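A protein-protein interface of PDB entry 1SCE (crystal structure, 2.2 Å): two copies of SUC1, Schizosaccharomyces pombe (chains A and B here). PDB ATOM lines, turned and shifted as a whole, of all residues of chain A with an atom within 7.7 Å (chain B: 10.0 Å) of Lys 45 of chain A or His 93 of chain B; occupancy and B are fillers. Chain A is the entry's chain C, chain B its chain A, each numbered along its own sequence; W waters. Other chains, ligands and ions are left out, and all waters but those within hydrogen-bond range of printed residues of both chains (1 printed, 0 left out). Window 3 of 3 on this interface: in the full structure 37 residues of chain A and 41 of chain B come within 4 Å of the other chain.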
ATOM      1  N   PHE A  21     -22.822  27.966 -16.096  1.00  0.00           N
ATOM      2  CA  PHE A  21     -23.296  27.434 -17.369  1.00  0.00           C
ATOM      3  C   PHE A  21     -22.379  26.399 -18.018  1.00  0.00           C
ATOM      4  O   PHE A  21     -22.835  25.544 -18.778  1.00  0.00           O
ATOM      5  CB  PHE A  21     -23.535  28.581 -18.354  1.00  0.00           C
ATOM      6  CG  PHE A  21     -24.742  29.402 -18.037  1.00  0.00           C
ATOM      7  CD1 PHE A  21     -26.015  28.833 -18.076  1.00  0.00           C
ATOM      8  CD2 PHE A  21     -24.617  30.743 -17.697  1.00  0.00           C
ATOM      9  CE1 PHE A  21     -27.151  29.592 -17.779  1.00  0.00           C
ATOM     10  CE2 PHE A  21     -25.742  31.513 -17.398  1.00  0.00           C
ATOM     11  CZ  PHE A  21     -27.016  30.937 -17.438  1.00  0.00           C
ATOM     12  N   HIS A  26     -23.078  20.893 -24.268  1.00  0.00           N
ATOM     13  CA  HIS A  26     -23.184  19.633 -24.989  1.00  0.00           C
ATOM     14  C   HIS A  26     -22.285  19.570 -26.219  1.00  0.00           C
ATOM     15  O   HIS A  26     -22.255  20.495 -27.025  1.00  0.00           O
ATOM     16  CB  HIS A  26     -24.658  19.410 -25.392  1.00  0.00           C
ATOM     17  CG  HIS A  26     -24.953  18.046 -25.944  1.00  0.00           C
ATOM     18  ND1 HIS A  26     -24.248  16.916 -25.582  1.00  0.00           N
ATOM     19  CD2 HIS A  26     -25.888  17.632 -26.832  1.00  0.00           C
ATOM     20  CE1 HIS A  26     -24.731  15.868 -26.224  1.00  0.00           C
ATOM     21  NE2 HIS A  26     -25.728  16.276 -26.989  1.00  0.00           N
ATOM     22  N   HIS A  40     -20.245  19.789 -33.431  1.00  0.00           N
ATOM     23  CA  HIS A  40     -21.268  20.819 -33.220  1.00  0.00           C
ATOM     24  C   HIS A  40     -21.346  20.960 -31.719  1.00  0.00           C
ATOM     25  O   HIS A  40     -21.533  19.962 -31.026  1.00  0.00           O
ATOM     26  CB  HIS A  40     -22.655  20.381 -33.724  1.00  0.00           C
ATOM     27  CG  HIS A  40     -22.706  20.025 -35.182  1.00  0.00           C
ATOM     28  ND1 HIS A  40     -23.686  19.214 -35.713  1.00  0.00           N
ATOM     29  CD2 HIS A  40     -21.888  20.348 -36.212  1.00  0.00           C
ATOM     30  CE1 HIS A  40     -23.470  19.048 -37.004  1.00  0.00           C
ATOM     31  NE2 HIS A  40     -22.384  19.725 -37.333  1.00  0.00           N
ATOM     32  N   VAL A  41     -21.187  22.180 -31.218  1.00  0.00           N
ATOM     33  CA  VAL A  41     -21.225  22.446 -29.781  1.00  0.00           C
ATOM     34  C   VAL A  41     -22.482  23.239 -29.461  1.00  0.00           C
ATOM     35  O   VAL A  41     -22.703  24.320 -30.018  1.00  0.00           O
ATOM     36  CB  VAL A  41     -19.974  23.257 -29.339  1.00  0.00           C
ATOM     37  CG1 VAL A  41     -20.060  23.624 -27.873  1.00  0.00           C
ATOM     38  CG2 VAL A  41     -18.712  22.457 -29.613  1.00  0.00           C
ATOM     39  N   MET A  42     -23.309  22.702 -28.575  1.00  0.00           N
ATOM     40  CA  MET A  42     -24.547  23.372 -28.220  1.00  0.00           C
ATOM     41  C   MET A  42     -24.480  23.910 -26.810  1.00  0.00           C
ATOM     42  O   MET A  42     -24.386  23.144 -25.850  1.00  0.00           O
ATOM     43  CB  MET A  42     -25.737  22.415 -28.354  1.00  0.00           C
ATOM     44  CG  MET A  42     -25.839  21.706 -29.713  1.00  0.00           C
ATOM     45  SD  MET A  42     -24.814  20.227 -29.776  1.00  0.00           S
ATOM     46  CE  MET A  42     -25.976  19.005 -30.260  1.00  0.00           C
ATOM     47  N   LEU A  43     -24.496  25.223 -26.667  1.00  0.00           N
ATOM     48  CA  LEU A  43     -24.453  25.794 -25.327  1.00  0.00           C
ATOM     49  C   LEU A  43     -25.846  26.184 -24.832  1.00  0.00           C
ATOM     50  O   LEU A  43     -26.749  26.420 -25.640  1.00  0.00           O
ATOM     51  CB  LEU A  43     -23.433  26.945 -25.219  1.00  0.00           C
ATOM     52  CG  LEU A  43     -22.989  27.865 -26.354  1.00  0.00           C
ATOM     53  CD1 LEU A  43     -23.989  28.980 -26.577  1.00  0.00           C
ATOM     54  CD2 LEU A  43     -21.657  28.463 -25.963  1.00  0.00           C
ATOM     55  N   PRO A  44     -26.059  26.182 -23.496  1.00  0.00           N
ATOM     56  CA  PRO A  44     -27.359  26.537 -22.920  1.00  0.00           C
ATOM     57  C   PRO A  44     -27.825  27.871 -23.477  1.00  0.00           C
ATOM     58  O   PRO A  44     -27.039  28.806 -23.592  1.00  0.00           O
ATOM     59  CB  PRO A  44     -27.056  26.639 -21.431  1.00  0.00           C
ATOM     60  CG  PRO A  44     -25.949  25.649 -21.241  1.00  0.00           C
ATOM     61  CD  PRO A  44     -25.070  25.937 -22.432  1.00  0.00           C
ATOM     62  N   LYS A  45     -29.101  27.946 -23.833  1.00  0.00           N
ATOM     63  CA  LYS A  45     -29.670  29.158 -24.397  1.00  0.00           C
ATOM     64  C   LYS A  45     -29.534  30.361 -23.480  1.00  0.00           C
ATOM     65  O   LYS A  45     -29.389  31.485 -23.948  1.00  0.00           O
ATOM     66  CB  LYS A  45     -31.138  28.929 -24.781  1.00  0.00           C
ATOM     67  CG  LYS A  45     -31.303  27.920 -25.922  1.00  0.00           C
ATOM     68  CD  LYS A  45     -32.762  27.676 -26.299  1.00  0.00           C
ATOM     69  CE  LYS A  45     -32.904  26.436 -27.195  1.00  0.00           C
ATOM     70  NZ  LYS A  45     -34.325  26.124 -27.558  1.00  0.00           N
ATOM     71  N   ALA A  46     -29.545  30.125 -22.175  1.00  0.00           N
ATOM     72  CA  ALA A  46     -29.433  31.211 -21.202  1.00  0.00           C
ATOM     73  C   ALA A  46     -28.022  31.792 -21.102  1.00  0.00           C
ATOM     74  O   ALA A  46     -27.845  32.962 -20.746  1.00  0.00           O
ATOM     75  CB  ALA A  46     -29.910  30.733 -19.840  1.00  0.00           C
ATOM     76  N   MET A  47     -27.024  30.976 -21.437  1.00  0.00           N
ATOM     77  CA  MET A  47     -25.631  31.395 -21.381  1.00  0.00           C
ATOM     78  C   MET A  47     -25.397  32.574 -22.304  1.00  0.00           C
ATOM     79  O   MET A  47     -24.546  33.418 -22.028  1.00  0.00           O
ATOM     80  CB  MET A  47     -24.711  30.238 -21.778  1.00  0.00           C
ATOM     81  CG  MET A  47     -23.223  30.503 -21.591  1.00  0.00           C
ATOM     82  SD  MET A  47     -22.185  29.139 -22.207  1.00  0.00           S
ATOM     83  CE  MET A  47     -20.564  29.615 -21.573  1.00  0.00           C
ATOM     84  N   LEU A  48     -26.181  32.654 -23.377  1.00  0.00           N
ATOM     85  CA  LEU A  48     -26.053  33.725 -24.371  1.00  0.00           C
ATOM     86  C   LEU A  48     -26.262  35.145 -23.829  1.00  0.00           C
ATOM     87  O   LEU A  48     -25.690  36.116 -24.348  1.00  0.00           O
ATOM     88  CB  LEU A  48     -27.007  33.471 -25.540  1.00  0.00           C
ATOM     89  CG  LEU A  48     -26.710  32.257 -26.425  1.00  0.00           C
ATOM     90  CD1 LEU A  48     -27.826  32.090 -27.438  1.00  0.00           C
ATOM     91  CD2 LEU A  48     -25.372  32.427 -27.127  1.00  0.00           C
ATOM     92  N   LYS A  49     -27.071  35.257 -22.781  1.00  0.00           N
ATOM     93  CA  LYS A  49     -27.371  36.543 -22.164  1.00  0.00           C
ATOM     94  C   LYS A  49     -26.200  37.061 -21.341  1.00  0.00           C
ATOM     95  O   LYS A  49     -26.108  38.259 -21.078  1.00  0.00           O
ATOM     96  CB  LYS A  49     -28.597  36.408 -21.265  1.00  0.00           C
ATOM     97  CG  LYS A  49     -29.608  37.535 -21.404  1.00  0.00           C
ATOM     98  CD  LYS A  49     -30.267  37.571 -22.789  1.00  0.00           C
ATOM     99  CE  LYS A  49     -30.991  36.266 -23.148  1.00  0.00           C
ATOM    100  NZ  LYS A  49     -30.109  35.257 -23.827  1.00  0.00           N
ATOM    101  N   ALA A  50     -25.317  36.156 -20.928  1.00  0.00           N
ATOM    102  CA  ALA A  50     -24.157  36.516 -20.114  1.00  0.00           C
ATOM    103  C   ALA A  50     -22.891  36.728 -20.935  1.00  0.00           C
ATOM    104  O   ALA A  50     -21.870  37.161 -20.401  1.00  0.00           O
ATOM    105  CB  ALA A  50     -23.918  35.451 -19.058  1.00  0.00           C
ATOM    106  N   ILE A  51     -22.946  36.392 -22.218  1.00  0.00           N
ATOM    107  CA  ILE A  51     -21.793  36.541 -23.100  1.00  0.00           C
ATOM    108  C   ILE A  51     -21.594  38.023 -23.448  1.00  0.00           C
ATOM    109  O   ILE A  51     -22.564  38.780 -23.516  1.00  0.00           O
ATOM    110  CB  ILE A  51     -21.961  35.662 -24.389  1.00  0.00           C
ATOM    111  CG1 ILE A  51     -21.922  34.172 -24.013  1.00  0.00           C
ATOM    112  CG2 ILE A  51     -20.864  35.968 -25.418  1.00  0.00           C
ATOM    113  CD1 ILE A  51     -22.097  33.196 -25.190  1.00  0.00           C
ATOM    114  N   PHE A  56     -20.541  38.853 -30.276  1.00  0.00           N
ATOM    115  CA  PHE A  56     -21.614  38.565 -31.222  1.00  0.00           C
ATOM    116  C   PHE A  56     -21.428  39.280 -32.551  1.00  0.00           C
ATOM    117  O   PHE A  56     -20.562  40.147 -32.688  1.00  0.00           O
ATOM    118  CB  PHE A  56     -22.966  38.957 -30.624  1.00  0.00           C
ATOM    119  CG  PHE A  56     -23.415  38.071 -29.507  1.00  0.00           C
ATOM    120  CD1 PHE A  56     -23.056  38.352 -28.194  1.00  0.00           C
ATOM    121  CD2 PHE A  56     -24.209  36.960 -29.764  1.00  0.00           C
ATOM    122  CE1 PHE A  56     -23.485  37.539 -27.153  1.00  0.00           C
ATOM    123  CE2 PHE A  56     -24.644  36.137 -28.731  1.00  0.00           C
ATOM    124  CZ  PHE A  56     -24.282  36.428 -27.423  1.00  0.00           C
ATOM    125  N   GLY A  61     -26.650  38.208 -35.852  1.00  0.00           N
ATOM    126  CA  GLY A  61     -27.080  38.013 -34.475  1.00  0.00           C
ATOM    127  C   GLY A  61     -26.581  36.709 -33.868  1.00  0.00           C
ATOM    128  O   GLY A  61     -27.145  36.198 -32.900  1.00  0.00           O
ATOM    129  N   THR A  62     -25.537  36.155 -34.467  1.00  0.00           N
ATOM    130  CA  THR A  62     -24.928  34.924 -33.997  1.00  0.00           C
ATOM    131  C   THR A  62     -23.579  35.324 -33.418  1.00  0.00           C
ATOM    132  O   THR A  62     -23.228  36.506 -33.420  1.00  0.00           O
ATOM    133  CB  THR A  62     -24.688  33.959 -35.171  1.00  0.00           C
ATOM    134  OG1 THR A  62     -23.798  34.565 -36.115  1.00  0.00           O
ATOM    135  CG2 THR A  62     -26.000  33.625 -35.869  1.00  0.00           C
ATOM    136  N   LEU A  63     -22.822  34.359 -32.909  1.00  0.00           N
ATOM    137  CA  LEU A  63     -21.500  34.666 -32.374  1.00  0.00           C
ATOM    138  C   LEU A  63     -20.557  34.799 -33.570  1.00  0.00           C
ATOM    139  O   LEU A  63     -20.718  34.104 -34.576  1.00  0.00           O
ATOM    140  CB  LEU A  63     -21.005  33.546 -31.444  1.00  0.00           C
ATOM    141  CG  LEU A  63     -21.720  33.234 -30.127  1.00  0.00           C
ATOM    142  CD1 LEU A  63     -20.937  32.178 -29.385  1.00  0.00           C
ATOM    143  CD2 LEU A  63     -21.809  34.461 -29.262  1.00  0.00           C
ATOM    144  N   VAL B  89     -28.326  27.868 -41.808  1.00  0.00           N
ATOM    145  CA  VAL B  89     -27.641  28.552 -40.725  1.00  0.00           C
ATOM    146  C   VAL B  89     -28.189  28.110 -39.370  1.00  0.00           C
ATOM    147  O   VAL B  89     -29.404  28.069 -39.153  1.00  0.00           O
ATOM    148  CB  VAL B  89     -27.776  30.095 -40.873  1.00  0.00           C
ATOM    149  CG1 VAL B  89     -27.192  30.820 -39.652  1.00  0.00           C
ATOM    150  CG2 VAL B  89     -27.038  30.567 -42.134  1.00  0.00           C
ATOM    151  N   PRO B  90     -27.300  27.716 -38.453  1.00  0.00           N
ATOM    152  CA  PRO B  90     -27.719  27.281 -37.118  1.00  0.00           C
ATOM    153  C   PRO B  90     -28.197  28.443 -36.248  1.00  0.00           C
ATOM    154  O   PRO B  90     -28.025  29.617 -36.598  1.00  0.00           O
ATOM    155  CB  PRO B  90     -26.443  26.663 -36.554  1.00  0.00           C
ATOM    156  CG  PRO B  90     -25.368  27.454 -37.219  1.00  0.00           C
ATOM    157  CD  PRO B  90     -25.858  27.499 -38.642  1.00  0.00           C
ATOM    158  N   GLU B  91     -28.838  28.102 -35.138  1.00  0.00           N
ATOM    159  CA  GLU B  91     -29.336  29.074 -34.171  1.00  0.00           C
ATOM    160  C   GLU B  91     -28.108  29.637 -33.427  1.00  0.00           C
ATOM    161  O   GLU B  91     -27.069  28.973 -33.376  1.00  0.00           O
ATOM    162  CB  GLU B  91     -30.279  28.368 -33.191  1.00  0.00           C
ATOM    163  CG  GLU B  91     -31.620  27.943 -33.784  1.00  0.00           C
ATOM    164  CD  GLU B  91     -31.479  27.070 -35.023  1.00  0.00           C
ATOM    165  OE1 GLU B  91     -30.959  25.928 -34.919  1.00  0.00           O
ATOM    166  OE2 GLU B  91     -31.891  27.537 -36.111  1.00  0.00           O
ATOM    167  N   PRO B  92     -28.239  30.813 -32.777  1.00  0.00           N
ATOM    168  CA  PRO B  92     -27.154  31.473 -32.035  1.00  0.00           C
ATOM    169  C   PRO B  92     -26.519  30.641 -30.930  1.00  0.00           C
ATOM    170  O   PRO B  92     -25.403  30.947 -30.492  1.00  0.00           O
ATOM    171  CB  PRO B  92     -27.835  32.708 -31.432  1.00  0.00           C
ATOM    172  CG  PRO B  92     -28.968  32.974 -32.342  1.00  0.00           C
ATOM    173  CD  PRO B  92     -29.486  31.581 -32.636  1.00  0.00           C
ATOM    174  N   HIS B  93     -27.215  29.612 -30.450  1.00  0.00           N
ATOM    175  CA  HIS B  93     -26.642  28.797 -29.383  1.00  0.00           C
ATOM    176  C   HIS B  93     -25.850  27.575 -29.850  1.00  0.00           C
ATOM    177  O   HIS B  93     -25.366  26.793 -29.028  1.00  0.00           O
ATOM    178  CB  HIS B  93     -27.701  28.411 -28.351  1.00  0.00           C
ATOM    179  CG  HIS B  93     -28.636  27.332 -28.802  1.00  0.00           C
ATOM    180  ND1 HIS B  93     -29.756  27.584 -29.565  1.00  0.00           N
ATOM    181  CD2 HIS B  93     -28.622  25.995 -28.580  1.00  0.00           C
ATOM    182  CE1 HIS B  93     -30.387  26.449 -29.801  1.00  0.00           C
ATOM    183  NE2 HIS B  93     -29.718  25.470 -29.216  1.00  0.00           N
ATOM    184  N   ILE B  94     -25.692  27.418 -31.162  1.00  0.00           N
ATOM    185  CA  ILE B  94     -24.939  26.287 -31.703  1.00  0.00           C
ATOM    186  C   ILE B  94     -23.734  26.833 -32.467  1.00  0.00           C
ATOM    187  O   ILE B  94     -23.881  27.700 -33.325  1.00  0.00           O
ATOM    188  CB  ILE B  94     -25.816  25.421 -32.643  1.00  0.00           C
ATOM    189  CG1 ILE B  94     -27.077  24.964 -31.911  1.00  0.00           C
ATOM    190  CG2 ILE B  94     -25.041  24.211 -33.129  1.00  0.00           C
ATOM    191  CD1 ILE B  94     -28.064  24.251 -32.800  1.00  0.00           C
ATOM    192  N   LEU B  95     -22.546  26.368 -32.096  1.00  0.00           N
ATOM    193  CA  LEU B  95     -21.289  26.778 -32.715  1.00  0.00           C
ATOM    194  C   LEU B  95     -20.721  25.574 -33.468  1.00  0.00           C
ATOM    195  O   LEU B  95     -20.718  24.457 -32.933  1.00  0.00           O
ATOM    196  CB  LEU B  95     -20.287  27.232 -31.644  1.00  0.00           C
ATOM    197  CG  LEU B  95     -20.740  28.121 -30.481  1.00  0.00           C
ATOM    198  CD1 LEU B  95     -19.509  28.661 -29.787  1.00  0.00           C
ATOM    199  CD2 LEU B  95     -21.608  29.265 -30.976  1.00  0.00           C
ATOM    200  N   LEU B  96     -20.199  25.809 -34.675  1.00  0.00           N
ATOM    201  CA  LEU B  96     -19.669  24.742 -35.533  1.00  0.00           C
ATOM    202  C   LEU B  96     -18.138  24.770 -35.626  1.00  0.00           C
ATOM    203  O   LEU B  96     -17.545  25.830 -35.833  1.00  0.00           O
ATOM    204  CB  LEU B  96     -20.278  24.864 -36.944  1.00  0.00           C
ATOM    205  CG  LEU B  96     -21.801  25.058 -37.123  1.00  0.00           C
ATOM    206  CD1 LEU B  96     -22.138  25.428 -38.587  1.00  0.00           C
ATOM    207  CD2 LEU B  96     -22.552  23.800 -36.702  1.00  0.00           C
ATOM    208  N   PHE B  97     -17.513  23.597 -35.535  1.00  0.00           N
ATOM    209  CA  PHE B  97     -16.054  23.459 -35.576  1.00  0.00           C
ATOM    210  C   PHE B  97     -15.610  22.423 -36.604  1.00  0.00           C
ATOM    211  O   PHE B  97     -16.392  21.556 -37.000  1.00  0.00           O
ATOM    212  CB  PHE B  97     -15.517  23.017 -34.204  1.00  0.00           C
ATOM    213  CG  PHE B  97     -15.645  24.052 -33.132  1.00  0.00           C
ATOM    214  CD1 PHE B  97     -14.687  25.053 -32.997  1.00  0.00           C
ATOM    215  CD2 PHE B  97     -16.731  24.038 -32.257  1.00  0.00           C
ATOM    216  CE1 PHE B  97     -14.811  26.030 -32.009  1.00  0.00           C
ATOM    217  CE2 PHE B  97     -16.864  25.016 -31.260  1.00  0.00           C
ATOM    218  CZ  PHE B  97     -15.906  26.011 -31.138  1.00  0.00           C
HETATM  219  O   HOH W   1     -23.536  31.568 -32.615  1.00  0.00           O
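O of His 93 of chain B sits at hydrogen-bond distance from N of Leu 43 of chain A (3.0 Å). The backbone carbonyl oxygen (O) of Leu 95 of chain B sits at hydrogen-bond distance from the backbone NH (N) of Val 41 of chain A, 2.9 Å away.
No position is printed for both chains.
Water W1 bridges O of Pro 92 of chain B and N of Leu 63 of chain A.
CA of His 40 of chain A touches O of Leu 95 of chain B, at 3.7 Å. His 40 of chain A touches Leu 96 of chain B (CD2 to CD2, 3.5 Å). O of Val 41 of chain A touches O of His 93 of chain B, 3.8 Å away. CA of Ile 94 of chain B touches O of Val 41 of chain A, at 3.4 Å. Phe 97 of chain B touches Val 41 of chain A (CE2 to CG2, 3.6 Å). His 93 of chain B touches Met 42 of chain A (O to CA, 3.6 Å). Lys 45 of chain A touches His 93 of chain B (CE to CE1, 3.6 Å). Leu 48 of chain A touches Pro 92 of chain B (CD2 to O, 3.7 Å). Leu 48 of chain A touches His 93 of chain B (CD1 to CB, 3.8 Å). Gly 61 of chain A touches Pro 92 of chain B.
The backbone carbonyl oxygen of His 26 of chain A sits at hydrogen-bond distance from the backbone NH of Met 42 of chain A (2.9 Å).
Phe 21 of chain A touches none of the printed residues of chain B. His 26 of chain A touches none of the printed residues of chain B. Printed residues of chain B within 4 Å of His 40 of chain A: Leu 95 (3.7 Å) and Leu 96 (3.5 Å). Of chain B, only His 93 comes within 4 Å of Leu 43 of chain A. Pro 44 of chain A touches none of the printed residues of chain B. Of chain B, only His 93 comes within 4 Å of Lys 45 of chain A. No residue of chain B comes within 4 Å of Ala 46 of chain A. Leu 48 of chain A touches just these residues of chain B: Pro 92 and His 93. His 93 of chain B touches just these residues of chain A: Val 41, Met 42, Leu 43, Lys 45 and Leu 48. Of the printed residues of chain A, Leu 95 of chain B touches His 40, Val 41 and Leu 63. The nearest residue of chain B that does not touch Lys 45 of chain A is Glu 91 of chain B (6.8 Å). The nearest residue of chain A that does not touch His 93 of chain B is Pro 44 of chain A (4.8 Å). The nearest printed residue of chain A that does not touch Pro 92 of chain B is Leu 63 of chain A (4.4 Å).
Printed residues of chain A that touch a printed residue of chain B: His 40, Val 41, Met 42, Leu 43, Lys 45, Leu 48, Gly 61 and Leu 63. Hydrophobic or aromatic side chains of chain A within 4 Å of the printed part of chain B: His 40, Val 41, Leu 43, Leu 48 and Leu 63. Hydrophobic or aromatic side chains of chain B within 4 Å of the printed part of chain A: Pro 92, His 93, Ile 94, Leu 95, Leu 96 and Phe 97. Among the printed residues, no Asp or Glu carboxylate lies within 4 Å of a Lys or Arg side-chain nitrogen of the other chain.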
